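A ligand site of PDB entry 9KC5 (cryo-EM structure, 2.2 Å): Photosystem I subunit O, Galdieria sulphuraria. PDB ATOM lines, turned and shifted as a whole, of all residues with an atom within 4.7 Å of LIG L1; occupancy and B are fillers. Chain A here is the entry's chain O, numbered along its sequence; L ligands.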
ATOM      1  N   VAL A  18     -12.147 -20.325   2.069  1.00  0.00           N
ATOM      2  CA  VAL A  18     -11.645 -19.379   1.094  1.00  0.00           C
ATOM      3  C   VAL A  18     -12.649 -18.241   0.923  1.00  0.00           C
ATOM      4  O   VAL A  18     -12.246 -17.074   0.832  1.00  0.00           O
ATOM      5  CB  VAL A  18     -11.321 -20.039  -0.264  1.00  0.00           C
ATOM      6  CG1 VAL A  18     -10.983 -19.013  -1.340  1.00  0.00           C
ATOM      7  CG2 VAL A  18     -10.184 -21.059  -0.148  1.00  0.00           C
ATOM      8  N   GLY A  22     -12.004 -14.503   1.795  1.00  0.00           N
ATOM      9  CA  GLY A  22     -12.167 -13.679   0.607  1.00  0.00           C
ATOM     10  C   GLY A  22     -13.112 -12.496   0.815  1.00  0.00           C
ATOM     11  O   GLY A  22     -12.942 -11.467   0.171  1.00  0.00           O
ATOM     12  N   TRP A  23     -14.117 -12.664   1.687  1.00  0.00           N
ATOM     13  CA  TRP A  23     -15.065 -11.605   1.992  1.00  0.00           C
ATOM     14  C   TRP A  23     -14.608 -10.773   3.185  1.00  0.00           C
ATOM     15  O   TRP A  23     -14.648  -9.541   3.133  1.00  0.00           O
ATOM     16  CB  TRP A  23     -16.465 -12.185   2.222  1.00  0.00           C
ATOM     17  CG  TRP A  23     -17.424 -11.204   2.853  1.00  0.00           C
ATOM     18  CD1 TRP A  23     -17.976 -11.287   4.092  1.00  0.00           C
ATOM     19  CD2 TRP A  23     -17.890  -9.963   2.283  1.00  0.00           C
ATOM     20  NE1 TRP A  23     -18.773 -10.199   4.326  1.00  0.00           N
ATOM     21  CE2 TRP A  23     -18.736  -9.360   3.240  1.00  0.00           C
ATOM     22  CE3 TRP A  23     -17.683  -9.295   1.068  1.00  0.00           C
ATOM     23  CZ2 TRP A  23     -19.372  -8.144   3.014  1.00  0.00           C
ATOM     24  CZ3 TRP A  23     -18.309  -8.088   0.847  1.00  0.00           C
ATOM     25  CH2 TRP A  23     -19.140  -7.517   1.816  1.00  0.00           C
ATOM     26  N   PRO A  26     -11.490  -7.842   2.616  1.00  0.00           N
ATOM     27  CA  PRO A  26     -11.847  -6.572   1.992  1.00  0.00           C
ATOM     28  C   PRO A  26     -12.997  -5.834   2.680  1.00  0.00           C
ATOM     29  O   PRO A  26     -13.063  -4.611   2.622  1.00  0.00           O
ATOM     30  CB  PRO A  26     -12.184  -6.956   0.555  1.00  0.00           C
ATOM     31  CG  PRO A  26     -12.558  -8.418   0.652  1.00  0.00           C
ATOM     32  CD  PRO A  26     -11.687  -8.992   1.718  1.00  0.00           C
ATOM     33  N   ALA A  27     -13.885  -6.577   3.349  1.00  0.00           N
ATOM     34  CA  ALA A  27     -14.986  -5.990   4.106  1.00  0.00           C
ATOM     35  C   ALA A  27     -14.502  -5.328   5.398  1.00  0.00           C
ATOM     36  O   ALA A  27     -15.281  -4.657   6.061  1.00  0.00           O
ATOM     37  CB  ALA A  27     -16.029  -7.047   4.407  1.00  0.00           C
ATOM     38  N   ILE A  29     -11.852  -3.222   5.314  1.00  0.00           N
ATOM     39  CA  ILE A  29     -11.303  -1.938   4.910  1.00  0.00           C
ATOM     40  C   ILE A  29     -12.189  -0.840   5.517  1.00  0.00           C
ATOM     41  O   ILE A  29     -13.404  -0.893   5.372  1.00  0.00           O
ATOM     42  CB  ILE A  29     -11.219  -1.822   3.370  1.00  0.00           C
ATOM     43  CG1 ILE A  29     -10.218  -2.822   2.781  1.00  0.00           C
ATOM     44  CG2 ILE A  29     -10.894  -0.388   2.923  1.00  0.00           C
ATOM     45  CD1 ILE A  29     -10.351  -3.026   1.288  1.00  0.00           C
ATOM     46  N   PRO A  30     -11.616   0.170   6.212  1.00  0.00           N
ATOM     47  CA  PRO A  30     -12.416   1.166   6.926  1.00  0.00           C
ATOM     48  C   PRO A  30     -13.205   2.114   6.023  1.00  0.00           C
ATOM     49  O   PRO A  30     -12.861   2.311   4.865  1.00  0.00           O
ATOM     50  CB  PRO A  30     -11.395   1.910   7.780  1.00  0.00           C
ATOM     51  CG  PRO A  30     -10.106   1.758   7.000  1.00  0.00           C
ATOM     52  CD  PRO A  30     -10.172   0.388   6.382  1.00  0.00           C
ATOM     53  N   SER A  31     -14.273   2.708   6.597  1.00  0.00           N
ATOM     54  CA  SER A  31     -15.175   3.618   5.911  1.00  0.00           C
ATOM     55  C   SER A  31     -15.334   4.906   6.702  1.00  0.00           C
ATOM     56  O   SER A  31     -14.982   4.964   7.882  1.00  0.00           O
ATOM     57  CB  SER A  31     -16.510   2.982   5.671  1.00  0.00           C
ATOM     58  OG  SER A  31     -17.476   3.965   5.332  1.00  0.00           O
ATOM     59  N   LEU A  36     -20.808   3.101  10.033  1.00  0.00           N
ATOM     60  CA  LEU A  36     -19.651   2.224  10.152  1.00  0.00           C
ATOM     61  C   LEU A  36     -18.555   2.848  11.022  1.00  0.00           C
ATOM     62  O   LEU A  36     -17.505   2.238  11.190  1.00  0.00           O
ATOM     63  CB  LEU A  36     -19.109   1.865   8.769  1.00  0.00           C
ATOM     64  CG  LEU A  36     -19.947   0.909   7.923  1.00  0.00           C
ATOM     65  CD1 LEU A  36     -19.134   0.517   6.700  1.00  0.00           C
ATOM     66  CD2 LEU A  36     -20.393  -0.342   8.661  1.00  0.00           C
ATOM     67  N   GLY A  40     -14.457  -0.756   9.219  1.00  0.00           N
ATOM     68  CA  GLY A  40     -15.132  -1.439   8.128  1.00  0.00           C
ATOM     69  C   GLY A  40     -16.360  -2.203   8.611  1.00  0.00           C
ATOM     70  O   GLY A  40     -16.682  -2.185   9.797  1.00  0.00           O
ATOM     71  N   LEU A  41     -17.033  -2.877   7.667  1.00  0.00           N
ATOM     72  CA  LEU A  41     -18.266  -3.593   7.931  1.00  0.00           C
ATOM     73  C   LEU A  41     -18.010  -4.788   8.854  1.00  0.00           C
ATOM     74  O   LEU A  41     -18.844  -5.103   9.696  1.00  0.00           O
ATOM     75  CB  LEU A  41     -18.893  -4.030   6.603  1.00  0.00           C
ATOM     76  CG  LEU A  41     -20.197  -4.838   6.682  1.00  0.00           C
ATOM     77  CD1 LEU A  41     -21.293  -4.098   7.429  1.00  0.00           C
ATOM     78  CD2 LEU A  41     -20.665  -5.197   5.278  1.00  0.00           C
ATOM     79  N   VAL A  80     -19.912 -14.290  -2.259  1.00  0.00           N
ATOM     80  CA  VAL A  80     -18.595 -14.888  -2.445  1.00  0.00           C
ATOM     81  C   VAL A  80     -18.711 -16.413  -2.351  1.00  0.00           C
ATOM     82  O   VAL A  80     -18.112 -17.110  -3.157  1.00  0.00           O
ATOM     83  CB  VAL A  80     -17.550 -14.323  -1.465  1.00  0.00           C
ATOM     84  CG1 VAL A  80     -16.192 -15.012  -1.597  1.00  0.00           C
ATOM     85  CG2 VAL A  80     -17.363 -12.822  -1.636  1.00  0.00           C
ATOM     86  N   TYR A  88     -15.463 -23.620  -7.901  1.00  0.00           N
ATOM     87  CA  TYR A  88     -14.964 -24.943  -7.555  1.00  0.00           C
ATOM     88  C   TYR A  88     -15.642 -26.014  -8.398  1.00  0.00           C
ATOM     89  O   TYR A  88     -15.014 -26.999  -8.777  1.00  0.00           O
ATOM     90  CB  TYR A  88     -15.176 -25.178  -6.050  1.00  0.00           C
ATOM     91  CG  TYR A  88     -14.619 -26.510  -5.572  1.00  0.00           C
ATOM     92  CD1 TYR A  88     -13.243 -26.678  -5.379  1.00  0.00           C
ATOM     93  CD2 TYR A  88     -15.443 -27.597  -5.321  1.00  0.00           C
ATOM     94  CE1 TYR A  88     -12.724 -27.883  -4.956  1.00  0.00           C
ATOM     95  CE2 TYR A  88     -14.932 -28.807  -4.893  1.00  0.00           C
ATOM     96  CZ  TYR A  88     -13.561 -28.952  -4.707  1.00  0.00           C
ATOM     97  OH  TYR A  88     -13.046 -30.148  -4.281  1.00  0.00           O
ATOM     98  N   SER A  91     -14.044 -26.205 -11.716  1.00  0.00           N
ATOM     99  CA  SER A  91     -12.748 -26.853 -11.604  1.00  0.00           C
ATOM    100  C   SER A  91     -12.893 -28.378 -11.514  1.00  0.00           C
ATOM    101  O   SER A  91     -12.020 -29.096 -11.988  1.00  0.00           O
ATOM    102  CB  SER A  91     -11.969 -26.317 -10.421  1.00  0.00           C
ATOM    103  OG  SER A  91     -12.532 -26.731  -9.185  1.00  0.00           O
HETATM  104  C1  LIG L   1     -11.211 -15.011  -4.115  1.00  0.00           C
HETATM  105  C2  LIG L   1     -12.379 -14.246  -4.389  1.00  0.00           C
HETATM  106  C3  LIG L   1     -11.131 -16.223  -5.067  1.00  0.00           C
HETATM  107  C4  LIG L   1     -15.996  -5.594  -1.439  1.00  0.00           C
HETATM  108  C5  LIG L   1     -12.777 -13.172  -3.347  1.00  0.00           C
HETATM  109  C6  LIG L   1      -8.501 -23.672  -4.613  1.00  0.00           C
HETATM  110  C7  LIG L   1      -8.303 -21.393  -6.335  1.00  0.00           C
HETATM  111  C8  LIG L   1      -9.283 -20.452  -6.358  1.00  0.00           C
HETATM  112  C9  LIG L   1      -8.958 -19.117  -5.621  1.00  0.00           C
HETATM  113  C10 LIG L   1     -13.338 -12.038  -3.914  1.00  0.00           C
HETATM  114  C11 LIG L   1      -9.971 -18.172  -5.903  1.00  0.00           C
HETATM  115  C12 LIG L   1      -9.870 -16.762  -5.260  1.00  0.00           C
HETATM  116  C13 LIG L   1     -19.001  -1.787   0.961  1.00  0.00           C
HETATM  117  C14 LIG L   1     -17.965  -2.502   1.840  1.00  0.00           C
HETATM  118  C15 LIG L   1     -17.690  -1.593   3.119  1.00  0.00           C
HETATM  119  C16 LIG L   1     -15.208  -9.837  -4.779  1.00  0.00           C
HETATM  120  C17 LIG L   1     -16.369  -2.008   3.851  1.00  0.00           C
HETATM  121  C18 LIG L   1     -15.190  -1.903   2.875  1.00  0.00           C
HETATM  122  C19 LIG L   1     -15.431  -2.596   1.567  1.00  0.00           C
HETATM  123  C20 LIG L   1     -16.671  -2.681   1.043  1.00  0.00           C
HETATM  124  C21 LIG L   1     -17.012  -5.451  -2.576  1.00  0.00           C
HETATM  125  C22 LIG L   1     -16.817  -3.599  -0.218  1.00  0.00           C
HETATM  126  C23 LIG L   1     -16.382  -4.897  -0.097  1.00  0.00           C
HETATM  127  C24 LIG L   1     -14.290 -11.274  -2.961  1.00  0.00           C
HETATM  128  C25 LIG L   1     -18.508  -3.856   2.324  1.00  0.00           C
HETATM  129  C26 LIG L   1     -14.580  -9.953  -3.385  1.00  0.00           C
HETATM  130  C27 LIG L   1     -15.307  -9.103  -2.308  1.00  0.00           C
HETATM  131  C28 LIG L   1     -15.132  -7.738  -2.462  1.00  0.00           C
HETATM  132  C29 LIG L   1     -15.588  -6.926  -1.213  1.00  0.00           C
HETATM  133  C30 LIG L   1     -14.369  -2.172   0.539  1.00  0.00           C
HETATM  134  C31 LIG L   1      -7.201 -22.083  -8.792  1.00  0.00           C
HETATM  135  C32 LIG L   1      -8.316 -22.983  -8.235  1.00  0.00           C
HETATM  136  C33 LIG L   1      -8.746 -22.740  -6.975  1.00  0.00           C
HETATM  137  C34 LIG L   1      -9.186 -23.812  -5.988  1.00  0.00           C
HETATM  138  C35 LIG L   1      -8.858 -25.253  -6.523  1.00  0.00           C
HETATM  139  C36 LIG L   1      -9.066 -25.401  -8.071  1.00  0.00           C
HETATM  140  C37 LIG L   1      -8.194 -24.365  -8.792  1.00  0.00           C
HETATM  141  O1  LIG L   1      -8.704 -26.667  -8.476  1.00  0.00           O
HETATM  142  C38 LIG L   1     -10.702 -23.734  -5.775  1.00  0.00           C
HETATM  143  O2  LIG L   1     -16.168  -1.177   4.934  1.00  0.00           O
HETATM  144  C39 LIG L   1     -11.025 -15.416  -2.631  1.00  0.00           C
HETATM  145  C40 LIG L   1      -8.577 -19.307  -4.135  1.00  0.00           C
HETATM  146 MG1  LG2 L   2     -14.612 -17.490  -9.185  1.00  0.00          MG
HETATM  147  C1  LG2 L   2     -13.774 -18.753 -12.286  1.00  0.00           C
HETATM  148  C2  LG2 L   2     -15.920 -14.760 -10.750  1.00  0.00           C
HETATM  149  C3  LG2 L   2     -15.078 -16.132  -6.117  1.00  0.00           C
HETATM  150  C4  LG2 L   2     -12.691 -20.250  -7.659  1.00  0.00           C
HETATM  151  N1  LG2 L   2     -14.784 -16.841 -11.152  1.00  0.00           N
HETATM  152  C5  LG2 L   2     -14.487 -17.443 -12.242  1.00  0.00           C
HETATM  153  C6  LG2 L   2     -14.905 -16.790 -13.535  1.00  0.00           C
HETATM  154  C7  LG2 L   2     -15.538 -15.506 -13.007  1.00  0.00           C
HETATM  155  C8  LG2 L   2     -15.411 -15.726 -11.537  1.00  0.00           C
HETATM  156  C9  LG2 L   2     -14.706 -14.305 -13.458  1.00  0.00           C
HETATM  157  C10 LG2 L   2     -15.919 -17.616 -14.373  1.00  0.00           C
HETATM  158  C11 LG2 L   2     -16.927 -18.514 -13.623  1.00  0.00           C
HETATM  159  C12 LG2 L   2     -17.991 -17.725 -12.884  1.00  0.00           C
HETATM  160  O1  LG2 L   2     -18.252 -17.926 -11.712  1.00  0.00           O
HETATM  161  O2  LG2 L   2     -18.743 -16.702 -13.589  1.00  0.00           O
HETATM  162  N2  LG2 L   2     -15.352 -15.691  -8.537  1.00  0.00           N
HETATM  163  C13 LG2 L   2     -15.906 -14.735  -9.276  1.00  0.00           C
HETATM  164  C14 LG2 L   2     -16.563 -13.629  -8.513  1.00  0.00           C
HETATM  165  C15 LG2 L   2     -16.299 -14.053  -7.112  1.00  0.00           C
HETATM  166  C16 LG2 L   2     -15.551 -15.345  -7.268  1.00  0.00           C
HETATM  167  C17 LG2 L   2     -17.265 -12.419  -9.074  1.00  0.00           C
HETATM  168  C18 LG2 L   2     -16.695 -13.462  -5.803  1.00  0.00           C
HETATM  169  C19 LG2 L   2     -17.575 -12.485  -5.711  1.00  0.00           C
HETATM  170  N3  LG2 L   2     -13.958 -18.060  -7.306  1.00  0.00           N
HETATM  171  C20 LG2 L   2     -14.338 -17.409  -6.192  1.00  0.00           C
HETATM  172  C21 LG2 L   2     -13.961 -18.062  -4.918  1.00  0.00           C
HETATM  173  C22 LG2 L   2     -13.252 -19.281  -5.376  1.00  0.00           C
HETATM  174  C23 LG2 L   2     -13.318 -19.168  -6.857  1.00  0.00           C
HETATM  175  C24 LG2 L   2     -14.227 -17.609  -3.510  1.00  0.00           C
HETATM  176  C25 LG2 L   2     -12.627 -20.349  -4.519  1.00  0.00           C
HETATM  177  C26 LG2 L   2     -13.647 -21.456  -4.348  1.00  0.00           C
HETATM  178  N4  LG2 L   2     -13.450 -19.074  -9.725  1.00  0.00           N
HETATM  179  C27 LG2 L   2     -12.797 -20.196  -9.114  1.00  0.00           C
HETATM  180  C28 LG2 L   2     -12.316 -21.246 -10.056  1.00  0.00           C
HETATM  181  C29 LG2 L   2     -12.727 -20.633 -11.356  1.00  0.00           C
HETATM  182  C30 LG2 L   2     -13.352 -19.440 -11.058  1.00  0.00           C
HETATM  183  C31 LG2 L   2     -11.606 -22.566  -9.937  1.00  0.00           C
HETATM  184  C32 LG2 L   2     -12.734 -20.793 -12.827  1.00  0.00           C
HETATM  185  O3  LG2 L   2     -12.248 -21.796 -13.462  1.00  0.00           O
HETATM  186  C33 LG2 L   2     -13.411 -19.621 -13.445  1.00  0.00           C
HETATM  187  C34 LG2 L   2     -12.493 -18.952 -14.435  1.00  0.00           C
HETATM  188  O4  LG2 L   2     -12.713 -19.032 -15.625  1.00  0.00           O
HETATM  189  O5  LG2 L   2     -11.319 -18.225 -13.988  1.00  0.00           O
HETATM  190  C35 LG2 L   2     -10.970 -16.950 -14.507  1.00  0.00           C
HETATM  191  C36 LG2 L   2     -19.281 -15.599 -12.876  1.00  0.00           C
HETATM  192  C37 LG2 L   2     -19.681 -14.561 -13.910  1.00  0.00           C
HETATM  193  C38 LG2 L   2     -19.333 -13.264 -13.882  1.00  0.00           C
HETATM  194  C39 LG2 L   2     -18.487 -12.680 -12.795  1.00  0.00           C
HETATM  195  C40 LG2 L   2     -19.805 -12.384 -15.005  1.00  0.00           C
HETATM  196  C41 LG2 L   2     -21.319 -12.324 -15.177  1.00  0.00           C
HETATM  197  C42 LG2 L   2     -21.948 -11.074 -14.578  1.00  0.00           C
HETATM  198  C43 LG2 L   2     -22.291 -11.062 -13.092  1.00  0.00           C
HETATM  199  C44 LG2 L   2     -22.484 -12.444 -12.468  1.00  0.00           C
HETATM  200  C45 LG2 L   2     -23.528 -10.169 -12.917  1.00  0.00           C
HETATM  201  C46 LG2 L   2     -24.284 -10.362 -11.596  1.00  0.00           C
HETATM  202  C47 LG2 L   2     -25.319  -9.288 -11.203  1.00  0.00           C
HETATM  203  C48 LG2 L   2     -25.569  -8.161 -12.219  1.00  0.00           C
HETATM  204 MG1  LG3 L   3     -15.559   6.072  -8.995  1.00  0.00          MG
HETATM  205  C1  LG3 L   3     -18.446   6.607  -7.213  1.00  0.00           C
HETATM  206  C2  LG3 L   3     -13.808   7.378  -6.376  1.00  0.00           C
HETATM  207  C3  LG3 L   3     -12.755   5.093 -10.595  1.00  0.00           C
HETATM  208  C4  LG3 L   3     -17.591   4.276 -11.537  1.00  0.00           C
HETATM  209  N1  LG3 L   3     -16.031   6.813  -7.106  1.00  0.00           N
HETATM  210  C5  LG3 L   3     -17.174   7.014  -6.565  1.00  0.00           C
HETATM  211  C6  LG3 L   3     -17.210   7.725  -5.241  1.00  0.00           C
HETATM  212  C7  LG3 L   3     -15.716   7.949  -4.995  1.00  0.00           C
HETATM  213  C8  LG3 L   3     -15.141   7.334  -6.250  1.00  0.00           C
HETATM  214  C9  LG3 L   3     -15.377   9.439  -4.881  1.00  0.00           C
HETATM  215  C10 LG3 L   3     -17.859   6.968  -4.067  1.00  0.00           C
HETATM  216  C11 LG3 L   3     -17.549   5.468  -4.034  1.00  0.00           C
HETATM  217  C12 LG3 L   3     -18.226   4.810  -2.849  1.00  0.00           C
HETATM  218  O1  LG3 L   3     -17.634   4.688  -1.786  1.00  0.00           O
HETATM  219  O2  LG3 L   3     -19.586   4.304  -2.966  1.00  0.00           O
HETATM  220  N2  LG3 L   3     -13.582   6.186  -8.535  1.00  0.00           N
HETATM  221  C13 LG3 L   3     -13.033   6.821  -7.490  1.00  0.00           C
HETATM  222  C14 LG3 L   3     -11.549   6.916  -7.513  1.00  0.00           C
HETATM  223  C15 LG3 L   3     -11.226   6.208  -8.799  1.00  0.00           C
HETATM  224  C16 LG3 L   3     -12.571   5.819  -9.318  1.00  0.00           C
HETATM  225  C17 LG3 L   3     -10.681   7.582  -6.476  1.00  0.00           C
HETATM  226  C18 LG3 L   3      -9.939   5.914  -9.496  1.00  0.00           C
HETATM  227  C19 LG3 L   3      -8.747   6.265  -9.051  1.00  0.00           C
HETATM  228  N3  LG3 L   3     -15.267   4.909 -10.681  1.00  0.00           N
HETATM  229  C20 LG3 L   3     -14.040   4.684 -11.184  1.00  0.00           C
HETATM  230  C21 LG3 L   3     -14.026   3.918 -12.470  1.00  0.00           C
HETATM  231  C22 LG3 L   3     -15.459   3.673 -12.748  1.00  0.00           C
HETATM  232  C23 LG3 L   3     -16.119   4.327 -11.578  1.00  0.00           C
HETATM  233  C24 LG3 L   3     -12.835   3.490 -13.288  1.00  0.00           C
HETATM  234  C25 LG3 L   3     -16.076   2.939 -13.920  1.00  0.00           C
HETATM  235  C26 LG3 L   3     -16.638   3.931 -14.912  1.00  0.00           C
HETATM  236  N4  LG3 L   3     -17.476   5.472  -9.342  1.00  0.00           N
HETATM  237  C27 LG3 L   3     -18.263   4.886 -10.386  1.00  0.00           C
HETATM  238  C28 LG3 L   3     -19.734   4.974 -10.217  1.00  0.00           C
HETATM  239  C29 LG3 L   3     -19.781   5.685  -8.909  1.00  0.00           C
HETATM  240  C30 LG3 L   3     -18.484   5.913  -8.508  1.00  0.00           C
HETATM  241  C31 LG3 L   3     -20.947   4.540 -10.982  1.00  0.00           C
HETATM  242  C32 LG3 L   3     -20.680   6.249  -7.866  1.00  0.00           C
HETATM  243  O3  LG3 L   3     -21.952   6.229  -7.907  1.00  0.00           O
HETATM  244  C33 LG3 L   3     -19.843   6.843  -6.784  1.00  0.00           C
HETATM  245  C34 LG3 L   3     -20.143   8.293  -6.652  1.00  0.00           C
HETATM  246  O4  LG3 L   3     -19.699   9.112  -7.453  1.00  0.00           O
HETATM  247  O5  LG3 L   3     -20.964   8.766  -5.582  1.00  0.00           O
HETATM  248  C35 LG3 L   3     -21.026  10.168  -5.353  1.00  0.00           C
HETATM  249  C36 LG3 L   3     -19.938   3.042  -2.420  1.00  0.00           C
HETATM  250  C37 LG3 L   3     -21.408   2.772  -2.635  1.00  0.00           C
HETATM  251  C38 LG3 L   3     -22.029   1.685  -2.135  1.00  0.00           C
HETATM  252  C39 LG3 L   3     -21.265   0.668  -1.329  1.00  0.00           C
HETATM  253  C40 LG3 L   3     -23.506   1.479  -2.380  1.00  0.00           C
HETATM  254  C41 LG3 L   3     -23.813   0.631  -3.609  1.00  0.00           C
HETATM  255  C42 LG3 L   3     -25.134   1.022  -4.305  1.00  0.00           C
HETATM  256  C43 LG3 L   3     -26.373   0.126  -4.116  1.00  0.00           C
HETATM  257  C44 LG3 L   3     -26.221  -1.079  -3.193  1.00  0.00           C
HETATM  258  C45 LG3 L   3     -26.895  -0.324  -5.483  1.00  0.00           C
HETATM  259 MG1  LG4 L   4     -24.599   3.901  -0.193  1.00  0.00          MG
HETATM  260  C1  LG4 L   4     -23.921   6.607  -2.236  1.00  0.00           C
HETATM  261  C2  LG4 L   4     -27.420   3.386  -1.982  1.00  0.00           C
HETATM  262  C3  LG4 L   4     -24.976   0.996   1.527  1.00  0.00           C
HETATM  263  C4  LG4 L   4     -21.209   4.256   1.178  1.00  0.00           C
HETATM  264  N1  LG4 L   4     -25.486   4.786  -1.842  1.00  0.00           N
HETATM  265  C5  LG4 L   4     -25.183   5.864  -2.470  1.00  0.00           C
HETATM  266  C6  LG4 L   4     -26.135   6.334  -3.530  1.00  0.00           C
HETATM  267  C7  LG4 L   4     -27.262   5.318  -3.390  1.00  0.00           C
HETATM  268  C8  LG4 L   4     -26.670   4.440  -2.329  1.00  0.00           C
HETATM  269  C9  LG4 L   4     -28.530   6.013  -2.890  1.00  0.00           C
HETATM  270  C10 LG4 L   4     -25.539   6.222  -4.944  1.00  0.00           C
HETATM  271  C11 LG4 L   4     -24.587   5.019  -5.120  1.00  0.00           C
HETATM  272  C12 LG4 L   4     -24.317   4.671  -6.565  1.00  0.00           C
HETATM  273  O1  LG4 L   4     -24.688   5.392  -7.495  1.00  0.00           O
HETATM  274  O2  LG4 L   4     -23.601   3.433  -6.893  1.00  0.00           O
HETATM  275  N2  LG4 L   4     -25.995   2.412  -0.219  1.00  0.00           N
HETATM  276  C13 LG4 L   4     -27.077   2.381  -0.980  1.00  0.00           C
HETATM  277  C14 LG4 L   4     -27.936   1.206  -0.780  1.00  0.00           C
HETATM  278  C15 LG4 L   4     -27.233   0.453   0.278  1.00  0.00           C
HETATM  279  C16 LG4 L   4     -26.031   1.308   0.548  1.00  0.00           C
HETATM  280  C17 LG4 L   4     -29.233   0.862  -1.445  1.00  0.00           C
HETATM  281  C18 LG4 L   4     -27.748  -0.839   0.781  1.00  0.00           C
HETATM  282  C19 LG4 L   4     -27.130  -1.668   1.590  1.00  0.00           C
HETATM  283  N3  LG4 L   4     -23.386   2.933   1.156  1.00  0.00           N
HETATM  284  C20 LG4 L   4     -23.709   1.733   1.683  1.00  0.00           C
HETATM  285  C21 LG4 L   4     -22.599   1.046   2.398  1.00  0.00           C
HETATM  286  C22 LG4 L   4     -21.483   2.020   2.302  1.00  0.00           C
HETATM  287  C23 LG4 L   4     -22.093   3.126   1.521  1.00  0.00           C
HETATM  288  C24 LG4 L   4     -22.570  -0.288   3.086  1.00  0.00           C
HETATM  289  C25 LG4 L   4     -20.073   1.847   2.792  1.00  0.00           C
HETATM  290  C26 LG4 L   4     -19.869   2.559   4.066  1.00  0.00           C
HETATM  291  N4  LG4 L   4     -22.906   5.020  -0.456  1.00  0.00           N
HETATM  292  C27 LG4 L   4     -21.646   5.221   0.182  1.00  0.00           C
HETATM  293  C28 LG4 L   4     -20.893   6.421  -0.225  1.00  0.00           C
HETATM  294  C29 LG4 L   4     -21.842   6.974  -1.223  1.00  0.00           C
HETATM  295  C30 LG4 L   4     -22.933   6.135  -1.263  1.00  0.00           C
HETATM  296  C31 LG4 L   4     -19.574   7.044   0.137  1.00  0.00           C
HETATM  297  C32 LG4 L   4     -22.097   8.085  -2.162  1.00  0.00           C
HETATM  298  O3  LG4 L   4     -21.313   9.068  -2.388  1.00  0.00           O
HETATM  299  C33 LG4 L   4     -23.396   7.867  -2.833  1.00  0.00           C
HETATM  300  C34 LG4 L   4     -24.255   9.060  -2.651  1.00  0.00           C
HETATM  301  O4  LG4 L   4     -24.502   9.510  -1.552  1.00  0.00           O
HETATM  302  O5  LG4 L   4     -24.776   9.731  -3.819  1.00  0.00           O
HETATM  303  C35 LG4 L   4     -25.987  10.476  -3.742  1.00  0.00           C
HETATM  304  C36 LG4 L   4     -22.265   3.136  -6.464  1.00  0.00           C
HETATM  305  C37 LG4 L   4     -21.666   2.080  -7.380  1.00  0.00           C
HETATM  306  C38 LG4 L   4     -20.389   1.650  -7.371  1.00  0.00           C
HETATM  307  C39 LG4 L   4     -20.036   0.588  -8.368  1.00  0.00           C
HETATM  308  C40 LG4 L   4     -19.308   2.150  -6.420  1.00  0.00           C
HETATM  309  C41 LG4 L   4     -18.025   2.626  -7.125  1.00  0.00           C
HETATM  310  C42 LG4 L   4     -16.783   1.820  -6.744  1.00  0.00           C
HETATM  311  C43 LG4 L   4     -15.507   2.470  -7.302  1.00  0.00           C
HETATM  312  C44 LG4 L   4     -14.475   1.410  -7.705  1.00  0.00           C
HETATM  313  C45 LG4 L   4     -14.976   3.532  -6.304  1.00  0.00           C
HETATM  314  C46 LG4 L   4     -13.770   3.136  -5.462  1.00  0.00           C
HETATM  315  C47 LG4 L   4     -13.556   4.084  -4.274  1.00  0.00           C
HETATM  316  C48 LG4 L   4     -12.146   4.663  -4.079  1.00  0.00           C
HETATM  317  C49 LG4 L   4     -10.984   3.751  -4.497  1.00  0.00           C
HETATM  318  C50 LG4 L   4     -11.981   5.074  -2.626  1.00  0.00           C
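The backbone carbonyl oxygen of Ile 29 lies within hydrogen-bond range of an oxygen (O2) of LIG L1 (2.8 Å). An oxygen (O2) of LIG L1 lies within hydrogen-bond range of the backbone NH (N) of Leu 41 (3.3 Å).
The backbone carbonyl oxygen (O) of Tyr 88 sits at hydrogen-bond distance from the side-chain hydroxyl (OG) of Ser 91. The backbone NH of Leu 41 sits at hydrogen-bond distance from the backbone carbonyl oxygen of Ala 27 (3.0 Å).
Residues that only touch LIG L1: Pro 26, Gly 40, Gly 22, Trp 23, Ala 27, Val 80, Val 18, Ser 91, Leu 36 and Tyr 88. 12 residues have an atom within 4 Å of LIG L1: Val 18, Gly 22, Trp 23, Pro 26, Ala 27, Ile 29, Leu 36, Gly 40, Leu 41, Val 80, Tyr 88 and Ser 91.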
